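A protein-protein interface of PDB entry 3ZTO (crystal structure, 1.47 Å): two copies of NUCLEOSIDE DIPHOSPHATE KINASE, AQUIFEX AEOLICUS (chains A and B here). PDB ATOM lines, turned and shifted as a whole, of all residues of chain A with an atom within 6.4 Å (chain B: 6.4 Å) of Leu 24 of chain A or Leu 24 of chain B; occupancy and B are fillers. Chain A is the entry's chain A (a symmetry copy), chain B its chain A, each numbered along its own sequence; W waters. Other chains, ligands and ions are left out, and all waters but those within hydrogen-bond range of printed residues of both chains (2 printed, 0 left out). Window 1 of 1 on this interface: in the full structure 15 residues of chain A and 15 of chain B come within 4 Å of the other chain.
Water W2 lies within hydrogen-bond range of OD1 of Asp 25 of chain A, N of Gly 21 of chain B and N of Lys 22 of chain B.
Water W1 lies within hydrogen-bond range of OD1 of Asp 25 of chain B (2.7 Å), N of Gly 21 of chain A (2.8 Å) and N of Lys 22 of chain A (3.0 Å).
OD1 of Asp 25 of chain A lies within salt-bridge range of NZ of Lys 22 of chain B.
The side-chain amino group (NZ) of Lys 22 of chain B sits close to the side-chain amide nitrogen (NE2) of Gln 29 of chain A.
The side-chain amino group of Lys 22 of chain A is in salt-bridge range of the side-chain carboxylate of Asp 25 of chain B (2.9 Å).
NZ of Lys 22 of chain A lies close to NE2 of Gln 29 of chain B (3.4 Å).
O of Gly 21 of chain A sits close to O of Gly 21 of chain B, 3.3 Å away.
Among the printed residues, merely in contact across the chains: Gly 21 of chain A with Asp 25 of chain B, Asp 25 of chain A with Gly 21 of chain B, Leu 24 of chain A with Leu 24 of chain B, Ile 28 of chain A with Gly 21 of chain B, Gly 21 of chain A with Ile 28 of chain B, Leu 20 of chain A with Leu 37 of chain B and Leu 37 of chain A with Leu 20 of chain B.
OD1 of Asp 25 of chain B lies within hydrogen-bond range of NE2 of Gln 29 of chain B (3.0 Å).
The side-chain carboxylate of Asp 25 of chain A sits at hydrogen-bond distance from the side-chain amide nitrogen of Gln 29 of chain A (3.0 Å).
Of the printed residues of chain B, Gln 29 of chain A touches Lys 22 (3.4 Å).
Printed residues of chain A within 4 Å of Leu 24 of chain B: Leu 24.
Of the printed residues of chain A, Asp 25 of chain B touches Gly 21 (3.8 Å) and Lys 22 (2.9 Å).
The nearest residue of chain B that does not touch Leu 24 of chain A is Gly 21 of chain B (4.2 Å).
Gly 21 of chain A touches its own counterpart, Gly 21 of chain B.
Gly 21 of chain A touches Asp 25 of chain B, and with the chains exchanged Asp 25 of chain A touches Gly 21 of chain B.
Lys 22 of chain A touches Gln 29 of chain B, and with the chains exchanged Gln 29 of chain A touches Lys 22 of chain B.
Leu 24 of chain B touches its own counterpart, Leu 24 of chain A.
Of the 18 printed residues of chain B, 8 touch a printed residue of chain A.
Hydrophobic or aromatic side chains of chain B within 4 Å of the printed part of chain A: Leu 20, Leu 24, Ile 28 and Leu 37.
Along chain B the printed residues that touch a printed residue of chain A span positions 20 to 37.
Of the 18 printed residues of chain A, 8 touch a printed residue of chain B.
Printed residues of chain A that touch a printed residue of chain B: Leu 20, Gly 21, Lys 22, Leu 24, Asp 25, Ile 28, Gln 29 and Leu 37.
Hydrophobic or aromatic side chains of chain A within 4 Å of the printed part of chain B: Leu 20, Leu 24, Ile 28 and Leu 37.
Among the printed residues, Asp or Glu carboxylates within 4 Å of a Lys or Arg side-chain nitrogen of the other chain: Lys 22 of chain A with Asp 25 of chain B and Asp 25 of chain A with Lys 22 of chain B.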
ATOM      1  N   ILE A   8     -25.946 -34.428 -16.460  1.00  0.00           N
ATOM      2  CA  ILE A   8     -25.349 -33.563 -17.459  1.00  0.00           C
ATOM      3  C   ILE A   8     -24.089 -34.209 -18.004  1.00  0.00           C
ATOM      4  O   ILE A   8     -23.408 -34.981 -17.323  1.00  0.00           O
ATOM      5  CB  ILE A   8     -24.996 -32.146 -16.937  1.00  0.00           C
ATOM      6  CG1 ILE A   8     -24.045 -32.208 -15.746  1.00  0.00           C
ATOM      7  CG2 ILE A   8     -26.259 -31.371 -16.584  1.00  0.00           C
ATOM      8  CD1 ILE A   8     -23.341 -30.882 -15.459  1.00  0.00           C
ATOM      9  N   VAL A  10     -20.755 -32.591 -20.122  1.00  0.00           N
ATOM     10  CA  VAL A  10     -20.028 -31.498 -20.758  1.00  0.00           C
ATOM     11  C   VAL A  10     -19.384 -32.053 -22.030  1.00  0.00           C
ATOM     12  O   VAL A  10     -18.592 -32.996 -21.984  1.00  0.00           O
ATOM     13  CB  VAL A  10     -18.988 -30.881 -19.799  1.00  0.00           C
ATOM     14  CG1 VAL A  10     -18.257 -29.728 -20.462  1.00  0.00           C
ATOM     15  CG2 VAL A  10     -19.699 -30.388 -18.522  1.00  0.00           C
ATOM     16  N   ALA A  19     -13.985 -24.755 -20.364  1.00  0.00           N
ATOM     17  CA  ALA A  19     -15.156 -24.315 -19.594  1.00  0.00           C
ATOM     18  C   ALA A  19     -15.614 -25.261 -18.489  1.00  0.00           C
ATOM     19  O   ALA A  19     -16.541 -24.950 -17.764  1.00  0.00           O
ATOM     20  CB  ALA A  19     -16.319 -24.069 -20.528  1.00  0.00           C
ATOM     21  N   LEU A  20     -14.976 -26.415 -18.352  1.00  0.00           N
ATOM     22  CA  LEU A  20     -15.466 -27.428 -17.410  1.00  0.00           C
ATOM     23  C   LEU A  20     -15.680 -26.884 -15.998  1.00  0.00           C
ATOM     24  O   LEU A  20     -16.722 -27.103 -15.390  1.00  0.00           O
ATOM     25  CB  LEU A  20     -14.505 -28.613 -17.323  1.00  0.00           C
ATOM     26  CG  LEU A  20     -14.892 -29.640 -16.265  1.00  0.00           C
ATOM     27  CD1 LEU A  20     -16.224 -30.326 -16.592  1.00  0.00           C
ATOM     28  CD2 LEU A  20     -13.795 -30.692 -16.169  1.00  0.00           C
ATOM     29  N   GLY A  21     -14.676 -26.196 -15.467  1.00  0.00           N
ATOM     30  CA  GLY A  21     -14.755 -25.736 -14.092  1.00  0.00           C
ATOM     31  C   GLY A  21     -15.831 -24.681 -13.928  1.00  0.00           C
ATOM     32  O   GLY A  21     -16.564 -24.684 -12.933  1.00  0.00           O
ATOM     33  N   LYS A  22     -15.935 -23.769 -14.893  1.00  0.00           N
ATOM     34  CA  LYS A  22     -16.945 -22.716 -14.828  1.00  0.00           C
ATOM     35  C   LYS A  22     -18.349 -23.319 -14.888  1.00  0.00           C
ATOM     36  O   LYS A  22     -19.269 -22.852 -14.209  1.00  0.00           O
ATOM     37  CB  LYS A  22     -16.749 -21.712 -15.964  1.00  0.00           C
ATOM     38  CG  LYS A  22     -15.472 -20.886 -15.836  1.00  0.00           C
ATOM     39  CD  LYS A  22     -15.411 -19.785 -16.903  1.00  0.00           C
ATOM     40  CE  LYS A  22     -14.176 -18.890 -16.765  1.00  0.00           C
ATOM     41  NZ  LYS A  22     -12.904 -19.591 -17.140  1.00  0.00           N
ATOM     42  N   ILE A  23     -18.513 -24.377 -15.682  1.00  0.00           N
ATOM     43  CA  ILE A  23     -19.823 -25.012 -15.804  1.00  0.00           C
ATOM     44  C   ILE A  23     -20.193 -25.712 -14.495  1.00  0.00           C
ATOM     45  O   ILE A  23     -21.314 -25.549 -13.995  1.00  0.00           O
ATOM     46  CB  ILE A  23     -19.860 -25.984 -16.997  1.00  0.00           C
ATOM     47  CG1 ILE A  23     -19.812 -25.177 -18.297  1.00  0.00           C
ATOM     48  CG2 ILE A  23     -21.111 -26.872 -16.916  1.00  0.00           C
ATOM     49  CD1 ILE A  23     -19.533 -26.001 -19.551  1.00  0.00           C
ATOM     50  N   LEU A  24     -19.262 -26.476 -13.918  1.00  0.00           N
ATOM     51  CA  LEU A  24     -19.554 -27.115 -12.642  1.00  0.00           C
ATOM     52  C   LEU A  24     -19.812 -26.085 -11.549  1.00  0.00           C
ATOM     53  O   LEU A  24     -20.729 -26.251 -10.744  1.00  0.00           O
ATOM     54  CB  LEU A  24     -18.425 -28.062 -12.232  1.00  0.00           C
ATOM     55  CG  LEU A  24     -18.198 -29.263 -13.149  1.00  0.00           C
ATOM     56  CD1 LEU A  24     -16.989 -30.053 -12.645  1.00  0.00           C
ATOM     57  CD2 LEU A  24     -19.431 -30.150 -13.206  1.00  0.00           C
ATOM     58  N   ASP A  25     -19.026 -25.008 -11.522  1.00  0.00           N
ATOM     59  CA  ASP A  25     -19.243 -23.946 -10.548  1.00  0.00           C
ATOM     60  C   ASP A  25     -20.665 -23.394 -10.616  1.00  0.00           C
ATOM     61  O   ASP A  25     -21.317 -23.149  -9.599  1.00  0.00           O
ATOM     62  CB  ASP A  25     -18.238 -22.812 -10.797  1.00  0.00           C
ATOM     63  CG  ASP A  25     -18.351 -21.702  -9.766  1.00  0.00           C
ATOM     64  OD1 ASP A  25     -18.384 -22.009  -8.560  1.00  0.00           O
ATOM     65  OD2 ASP A  25     -18.429 -20.518 -10.147  1.00  0.00           O
ATOM     66  N   ARG A  26     -21.174 -23.172 -11.825  1.00  0.00           N
ATOM     67  CA  ARG A  26     -22.529 -22.655 -11.970  1.00  0.00           C
ATOM     68  C   ARG A  26     -23.560 -23.567 -11.324  1.00  0.00           C
ATOM     69  O   ARG A  26     -24.435 -23.102 -10.586  1.00  0.00           O
ATOM     70  CB  ARG A  26     -22.861 -22.465 -13.453  1.00  0.00           C
ATOM     71  CG  ARG A  26     -24.281 -22.006 -13.721  1.00  0.00           C
ATOM     72  CD  ARG A  26     -24.625 -20.666 -13.037  1.00  0.00           C
ATOM     73  NE  ARG A  26     -25.916 -20.202 -13.524  1.00  0.00           N
ATOM     74  CZ  ARG A  26     -26.087 -19.693 -14.742  1.00  0.00           C
ATOM     75  NH1 ARG A  26     -25.051 -19.535 -15.542  1.00  0.00           N
ATOM     76  NH2 ARG A  26     -27.290 -19.336 -15.142  1.00  0.00           N
ATOM     77  N   PHE A  27     -23.480 -24.867 -11.593  1.00  0.00           N
ATOM     78  CA  PHE A  27     -24.489 -25.746 -11.021  1.00  0.00           C
ATOM     79  C   PHE A  27     -24.359 -25.840  -9.508  1.00  0.00           C
ATOM     80  O   PHE A  27     -25.357 -25.944  -8.807  1.00  0.00           O
ATOM     81  CB  PHE A  27     -24.441 -27.127 -11.685  1.00  0.00           C
ATOM     82  CG  PHE A  27     -24.968 -27.112 -13.088  1.00  0.00           C
ATOM     83  CD1 PHE A  27     -26.313 -26.856 -13.318  1.00  0.00           C
ATOM     84  CD2 PHE A  27     -24.128 -27.313 -14.168  1.00  0.00           C
ATOM     85  CE1 PHE A  27     -26.806 -26.822 -14.599  1.00  0.00           C
ATOM     86  CE2 PHE A  27     -24.629 -27.259 -15.454  1.00  0.00           C
ATOM     87  CZ  PHE A  27     -25.951 -27.013 -15.668  1.00  0.00           C
ATOM     88  N   ILE A  28     -23.135 -25.776  -9.005  1.00  0.00           N
ATOM     89  CA  ILE A  28     -22.935 -25.765  -7.559  1.00  0.00           C
ATOM     90  C   ILE A  28     -23.558 -24.506  -6.948  1.00  0.00           C
ATOM     91  O   ILE A  28     -24.240 -24.571  -5.922  1.00  0.00           O
ATOM     92  CB  ILE A  28     -21.442 -25.833  -7.220  1.00  0.00           C
ATOM     93  CG1 ILE A  28     -20.863 -27.186  -7.616  1.00  0.00           C
ATOM     94  CG2 ILE A  28     -21.225 -25.593  -5.732  1.00  0.00           C
ATOM     95  CD1 ILE A  28     -19.337 -27.199  -7.670  1.00  0.00           C
ATOM     96  N   GLN A  29     -23.338 -23.361  -7.569  1.00  0.00           N
ATOM     97  CA  GLN A  29     -23.854 -22.114  -7.009  1.00  0.00           C
ATOM     98  C   GLN A  29     -25.379 -22.006  -7.099  1.00  0.00           C
ATOM     99  O   GLN A  29     -26.000 -21.334  -6.274  1.00  0.00           O
ATOM    100  CB  GLN A  29     -23.208 -20.903  -7.666  1.00  0.00           C
ATOM    101  CG  GLN A  29     -21.680 -20.809  -7.462  1.00  0.00           C
ATOM    102  CD  GLN A  29     -21.209 -21.281  -6.093  1.00  0.00           C
ATOM    103  OE1 GLN A  29     -21.831 -21.009  -5.061  1.00  0.00           O
ATOM    104  NE2 GLN A  29     -20.091 -22.004  -6.083  1.00  0.00           N
ATOM    105  N   ILE A  34     -23.678 -32.313  -6.431  1.00  0.00           N
ATOM    106  CA  ILE A  34     -23.072 -33.249  -7.367  1.00  0.00           C
ATOM    107  C   ILE A  34     -22.960 -34.607  -6.666  1.00  0.00           C
ATOM    108  O   ILE A  34     -22.263 -34.741  -5.656  1.00  0.00           O
ATOM    109  CB  ILE A  34     -21.695 -32.758  -7.839  1.00  0.00           C
ATOM    110  CG1 ILE A  34     -21.864 -31.415  -8.555  1.00  0.00           C
ATOM    111  CG2 ILE A  34     -21.019 -33.793  -8.753  1.00  0.00           C
ATOM    112  CD1 ILE A  34     -20.531 -30.761  -8.911  1.00  0.00           C
ATOM    113  N   LEU A  37     -19.504 -37.900 -10.556  1.00  0.00           N
ATOM    114  CA  LEU A  37     -18.733 -37.081 -11.483  1.00  0.00           C
ATOM    115  C   LEU A  37     -17.582 -37.893 -12.040  1.00  0.00           C
ATOM    116  O   LEU A  37     -16.858 -38.506 -11.287  1.00  0.00           O
ATOM    117  CB  LEU A  37     -18.167 -35.851 -10.745  1.00  0.00           C
ATOM    118  CG  LEU A  37     -17.268 -34.913 -11.556  1.00  0.00           C
ATOM    119  CD1 LEU A  37     -18.138 -34.085 -12.475  1.00  0.00           C
ATOM    120  CD2 LEU A  37     -16.453 -33.997 -10.628  1.00  0.00           C
ATOM    121  N   VAL A  73     -17.169 -35.046 -19.645  1.00  0.00           N
ATOM    122  CA  VAL A  73     -17.361 -35.189 -18.201  1.00  0.00           C
ATOM    123  C   VAL A  73     -18.845 -35.253 -17.891  1.00  0.00           C
ATOM    124  O   VAL A  73     -19.616 -34.399 -18.306  1.00  0.00           O
ATOM    125  CB  VAL A  73     -16.730 -34.031 -17.424  1.00  0.00           C
ATOM    126  CG1 VAL A  73     -17.127 -34.067 -15.970  1.00  0.00           C
ATOM    127  CG2 VAL A  73     -15.245 -34.085 -17.562  1.00  0.00           C
ATOM    128  N   ALA A  75     -21.933 -35.637 -14.898  1.00  0.00           N
ATOM    129  CA  ALA A  75     -22.207 -35.435 -13.486  1.00  0.00           C
ATOM    130  C   ALA A  75     -23.664 -35.703 -13.221  1.00  0.00           C
ATOM    131  O   ALA A  75     -24.513 -35.412 -14.059  1.00  0.00           O
ATOM    132  CB  ALA A  75     -21.869 -34.005 -13.061  1.00  0.00           C
ATOM    133  N   LEU A  77     -26.613 -34.451 -10.979  1.00  0.00           N
ATOM    134  CA  LEU A  77     -27.022 -33.316 -10.169  1.00  0.00           C
ATOM    135  C   LEU A  77     -28.333 -33.615  -9.460  1.00  0.00           C
ATOM    136  O   LEU A  77     -29.283 -34.070 -10.075  1.00  0.00           O
ATOM    137  CB  LEU A  77     -27.211 -32.066 -11.050  1.00  0.00           C
ATOM    138  CG  LEU A  77     -26.008 -31.688 -11.909  1.00  0.00           C
ATOM    139  CD1 LEU A  77     -26.311 -30.453 -12.756  1.00  0.00           C
ATOM    140  CD2 LEU A  77     -24.809 -31.426 -11.009  1.00  0.00           C
ATOM    141  N   ILE B   8      -4.121 -34.231  -7.976  1.00  0.00           N
ATOM    142  CA  ILE B   8      -4.743 -33.420  -6.948  1.00  0.00           C
ATOM    143  C   ILE B   8      -5.982 -34.124  -6.427  1.00  0.00           C
ATOM    144  O   ILE B   8      -6.639 -34.893  -7.135  1.00  0.00           O
ATOM    145  CB  ILE B   8      -5.141 -31.998  -7.421  1.00  0.00           C
ATOM    146  CG1 ILE B   8      -6.091 -32.048  -8.614  1.00  0.00           C
ATOM    147  CG2 ILE B   8      -3.903 -31.171  -7.747  1.00  0.00           C
ATOM    148  CD1 ILE B   8      -6.836 -30.736  -8.856  1.00  0.00           C
ATOM    149  N   VAL B  10      -9.364 -32.686  -4.256  1.00  0.00           N
ATOM    150  CA  VAL B  10     -10.126 -31.639  -3.583  1.00  0.00           C
ATOM    151  C   VAL B  10     -10.751 -32.257  -2.331  1.00  0.00           C
ATOM    152  O   VAL B  10     -11.512 -33.223  -2.411  1.00  0.00           O
ATOM    153  CB  VAL B  10     -11.185 -31.022  -4.520  1.00  0.00           C
ATOM    154  CG1 VAL B  10     -11.951 -29.917  -3.818  1.00  0.00           C
ATOM    155  CG2 VAL B  10     -10.491 -30.463  -5.779  1.00  0.00           C
ATOM    156  N   ALA B  19     -16.378 -25.081  -3.747  1.00  0.00           N
ATOM    157  CA  ALA B  19     -15.222 -24.577  -4.501  1.00  0.00           C
ATOM    158  C   ALA B  19     -14.735 -25.469  -5.637  1.00  0.00           C
ATOM    159  O   ALA B  19     -13.818 -25.104  -6.351  1.00  0.00           O
ATOM    160  CB  ALA B  19     -14.067 -24.327  -3.558  1.00  0.00           C
ATOM    161  N   LEU B  20     -15.336 -26.638  -5.815  1.00  0.00           N
ATOM    162  CA  LEU B  20     -14.815 -27.601  -6.791  1.00  0.00           C
ATOM    163  C   LEU B  20     -14.619 -27.003  -8.183  1.00  0.00           C
ATOM    164  O   LEU B  20     -13.571 -27.168  -8.797  1.00  0.00           O
ATOM    165  CB  LEU B  20     -15.738 -28.813  -6.919  1.00  0.00           C
ATOM    166  CG  LEU B  20     -15.319 -29.789  -8.012  1.00  0.00           C
ATOM    167  CD1 LEU B  20     -13.966 -30.444  -7.708  1.00  0.00           C
ATOM    168  CD2 LEU B  20     -16.383 -30.871  -8.144  1.00  0.00           C
ATOM    169  N   GLY B  21     -15.645 -26.329  -8.690  1.00  0.00           N
ATOM    170  CA  GLY B  21     -15.581 -25.819 -10.048  1.00  0.00           C
ATOM    171  C   GLY B  21     -14.539 -24.725 -10.176  1.00  0.00           C
ATOM    172  O   GLY B  21     -13.807 -24.672 -11.169  1.00  0.00           O
ATOM    173  N   LYS B  22     -14.463 -23.845  -9.179  1.00  0.00           N
ATOM    174  CA  LYS B  22     -13.487 -22.759  -9.207  1.00  0.00           C
ATOM    175  C   LYS B  22     -12.065 -23.319  -9.167  1.00  0.00           C
ATOM    176  O   LYS B  22     -11.160 -22.799  -9.830  1.00  0.00           O
ATOM    177  CB  LYS B  22     -13.714 -21.801  -8.038  1.00  0.00           C
ATOM    178  CG  LYS B  22     -15.016 -21.012  -8.137  1.00  0.00           C
ATOM    179  CD  LYS B  22     -15.111 -19.951  -7.033  1.00  0.00           C
ATOM    180  CE  LYS B  22     -16.374 -19.091  -7.141  1.00  0.00           C
ATOM    181  NZ  LYS B  22     -17.623 -19.844  -6.791  1.00  0.00           N
ATOM    182  N   ILE B  23     -11.867 -24.398  -8.410  1.00  0.00           N
ATOM    183  CA  ILE B  23     -10.538 -24.996  -8.310  1.00  0.00           C
ATOM    184  C   ILE B  23     -10.146 -25.638  -9.641  1.00  0.00           C
ATOM    185  O   ILE B  23      -9.031 -25.422 -10.135  1.00  0.00           O
ATOM    186  CB  ILE B  23     -10.470 -26.006  -7.151  1.00  0.00           C
ATOM    187  CG1 ILE B  23     -10.542 -25.247  -5.824  1.00  0.00           C
ATOM    188  CG2 ILE B  23      -9.191 -26.851  -7.262  1.00  0.00           C
ATOM    189  CD1 ILE B  23     -10.794 -26.122  -4.599  1.00  0.00           C
ATOM    190  N   LEU B  24     -11.053 -26.411 -10.245  1.00  0.00           N
ATOM    191  CA  LEU B  24     -10.742 -26.995 -11.543  1.00  0.00           C
ATOM    192  C   LEU B  24     -10.517 -25.920 -12.599  1.00  0.00           C
ATOM    193  O   LEU B  24      -9.596 -26.030 -13.409  1.00  0.00           O
ATOM    194  CB  LEU B  24     -11.840 -27.962 -11.985  1.00  0.00           C
ATOM    195  CG  LEU B  24     -12.029 -29.201 -11.111  1.00  0.00           C
ATOM    196  CD1 LEU B  24     -13.213 -30.010 -11.643  1.00  0.00           C
ATOM    197  CD2 LEU B  24     -10.769 -30.051 -11.084  1.00  0.00           C
ATOM    198  N   ASP B  25     -11.337 -24.868 -12.589  1.00  0.00           N
ATOM    199  CA  ASP B  25     -11.154 -23.767 -13.526  1.00  0.00           C
ATOM    200  C   ASP B  25      -9.749 -23.173 -13.438  1.00  0.00           C
ATOM    201  O   ASP B  25      -9.106 -22.872 -14.446  1.00  0.00           O
ATOM    202  CB  ASP B  25     -12.194 -22.675 -13.238  1.00  0.00           C
ATOM    203  CG  ASP B  25     -12.116 -21.526 -14.230  1.00  0.00           C
ATOM    204  OD1 ASP B  25     -12.074 -21.790 -15.446  1.00  0.00           O
ATOM    205  OD2 ASP B  25     -12.076 -20.354 -13.809  1.00  0.00           O
ATOM    206  N   ARG B  26      -9.247 -22.977 -12.222  1.00  0.00           N
ATOM    207  CA  ARG B  26      -7.909 -22.423 -12.058  1.00  0.00           C
ATOM    208  C   ARG B  26      -6.850 -23.279 -12.735  1.00  0.00           C
ATOM    209  O   ARG B  26      -5.990 -22.761 -13.456  1.00  0.00           O
ATOM    210  CB  ARG B  26      -7.583 -22.274 -10.570  1.00  0.00           C
ATOM    211  CG  ARG B  26      -6.177 -21.780 -10.285  1.00  0.00           C
ATOM    212  CD  ARG B  26      -5.876 -20.407 -10.922  1.00  0.00           C
ATOM    213  NE  ARG B  26      -4.601 -19.920 -10.419  1.00  0.00           N
ATOM    214  CZ  ARG B  26      -4.445 -19.448  -9.184  1.00  0.00           C
ATOM    215  NH1 ARG B  26      -5.484 -19.350  -8.380  1.00  0.00           N
ATOM    216  NH2 ARG B  26      -3.254 -19.067  -8.771  1.00  0.00           N
ATOM    217  N   PHE B  27      -6.889 -24.589 -12.512  1.00  0.00           N
ATOM    218  CA  PHE B  27      -5.853 -25.416 -13.112  1.00  0.00           C
ATOM    219  C   PHE B  27      -5.981 -25.462 -14.629  1.00  0.00           C
ATOM    220  O   PHE B  27      -4.981 -25.510 -15.332  1.00  0.00           O
ATOM    221  CB  PHE B  27      -5.857 -26.820 -12.497  1.00  0.00           C
ATOM    222  CG  PHE B  27      -5.330 -26.837 -11.093  1.00  0.00           C
ATOM    223  CD1 PHE B  27      -3.994 -26.547 -10.854  1.00  0.00           C
ATOM    224  CD2 PHE B  27      -6.163 -27.102 -10.022  1.00  0.00           C
ATOM    225  CE1 PHE B  27      -3.501 -26.541  -9.573  1.00  0.00           C
ATOM    226  CE2 PHE B  27      -5.663 -27.076  -8.735  1.00  0.00           C
ATOM    227  CZ  PHE B  27      -4.350 -26.796  -8.512  1.00  0.00           C
ATOM    228  N   ILE B  28      -7.207 -25.419 -15.130  1.00  0.00           N
ATOM    229  CA  ILE B  28      -7.408 -25.364 -16.574  1.00  0.00           C
ATOM    230  C   ILE B  28      -6.825 -24.066 -17.141  1.00  0.00           C
ATOM    231  O   ILE B  28      -6.142 -24.073 -18.168  1.00  0.00           O
ATOM    232  CB  ILE B  28      -8.898 -25.467 -16.916  1.00  0.00           C
ATOM    233  CG1 ILE B  28      -9.433 -26.851 -16.567  1.00  0.00           C
ATOM    234  CG2 ILE B  28      -9.123 -25.183 -18.395  1.00  0.00           C
ATOM    235  CD1 ILE B  28     -10.958 -26.914 -16.515  1.00  0.00           C
ATOM    236  N   GLN B  29      -7.081 -22.950 -16.481  1.00  0.00           N
ATOM    237  CA  GLN B  29      -6.605 -21.669 -16.997  1.00  0.00           C
ATOM    238  C   GLN B  29      -5.084 -21.516 -16.902  1.00  0.00           C
ATOM    239  O   GLN B  29      -4.485 -20.798 -17.703  1.00  0.00           O
ATOM    240  CB  GLN B  29      -7.287 -20.503 -16.299  1.00  0.00           C
ATOM    241  CG  GLN B  29      -8.819 -20.450 -16.501  1.00  0.00           C
ATOM    242  CD  GLN B  29      -9.275 -20.889 -17.885  1.00  0.00           C
ATOM    243  OE1 GLN B  29      -8.663 -20.561 -18.907  1.00  0.00           O
ATOM    244  NE2 GLN B  29     -10.369 -21.646 -17.920  1.00  0.00           N
ATOM    245  N   ILE B  34      -6.459 -31.843 -17.928  1.00  0.00           N
ATOM    246  CA  ILE B  34      -7.035 -32.829 -17.024  1.00  0.00           C
ATOM    247  C   ILE B  34      -7.104 -34.165 -17.772  1.00  0.00           C
ATOM    248  O   ILE B  34      -7.797 -34.286 -18.787  1.00  0.00           O
ATOM    249  CB  ILE B  34      -8.426 -32.398 -16.537  1.00  0.00           C
ATOM    250  CG1 ILE B  34      -8.299 -31.076 -15.775  1.00  0.00           C
ATOM    251  CG2 ILE B  34      -9.069 -33.485 -15.659  1.00  0.00           C
ATOM    252  CD1 ILE B  34      -9.652 -30.477 -15.397  1.00  0.00           C
ATOM    253  N   LEU B  37     -10.452 -37.697 -14.001  1.00  0.00           N
ATOM    254  CA  LEU B  37     -11.249 -36.936 -13.046  1.00  0.00           C
ATOM    255  C   LEU B  37     -12.374 -37.802 -12.518  1.00  0.00           C
ATOM    256  O   LEU B  37     -13.077 -38.412 -13.292  1.00  0.00           O
ATOM    257  CB  LEU B  37     -11.853 -35.699 -13.742  1.00  0.00           C
ATOM    258  CG  LEU B  37     -12.781 -34.819 -12.899  1.00  0.00           C
ATOM    259  CD1 LEU B  37     -11.937 -33.996 -11.951  1.00  0.00           C
ATOM    260  CD2 LEU B  37     -13.625 -33.898 -13.796  1.00  0.00           C
ATOM    261  N   VAL B  73     -12.871 -35.234  -4.820  1.00  0.00           N
ATOM    262  CA  VAL B  73     -12.676 -35.321  -6.267  1.00  0.00           C
ATOM    263  C   VAL B  73     -11.191 -35.328  -6.578  1.00  0.00           C
ATOM    264  O   VAL B  73     -10.447 -34.465  -6.134  1.00  0.00           O
ATOM    265  CB  VAL B  73     -13.343 -34.158  -7.004  1.00  0.00           C
ATOM    266  CG1 VAL B  73     -12.947 -34.131  -8.458  1.00  0.00           C
ATOM    267  CG2 VAL B  73     -14.826 -34.264  -6.869  1.00  0.00           C
ATOM    268  N   ALA B  75      -8.093 -35.511  -9.581  1.00  0.00           N
ATOM    269  CA  ALA B  75      -7.827 -35.251 -10.986  1.00  0.00           C
ATOM    270  C   ALA B  75      -6.363 -35.465 -11.259  1.00  0.00           C
ATOM    271  O   ALA B  75      -5.523 -35.176 -10.411  1.00  0.00           O
ATOM    272  CB  ALA B  75      -8.211 -33.819 -11.361  1.00  0.00           C
ATOM    273  N   LEU B  77      -3.456 -34.043 -13.454  1.00  0.00           N
ATOM    274  CA  LEU B  77      -3.084 -32.868 -14.225  1.00  0.00           C
ATOM    275  C   LEU B  77      -1.764 -33.101 -14.943  1.00  0.00           C
ATOM    276  O   LEU B  77      -0.799 -33.547 -14.343  1.00  0.00           O
ATOM    277  CB  LEU B  77      -2.933 -31.644 -13.301  1.00  0.00           C
ATOM    278  CG  LEU B  77      -4.147 -31.334 -12.429  1.00  0.00           C
ATOM    279  CD1 LEU B  77      -3.883 -30.120 -11.541  1.00  0.00           C
ATOM    280  CD2 LEU B  77      -5.354 -31.079 -13.321  1.00  0.00           C
HETATM  281  O   HOH W   1     -13.343 -23.920 -16.482  1.00  0.00           O
HETATM  282  O   HOH W   2     -17.048 -24.132  -7.598  1.00  0.00           O
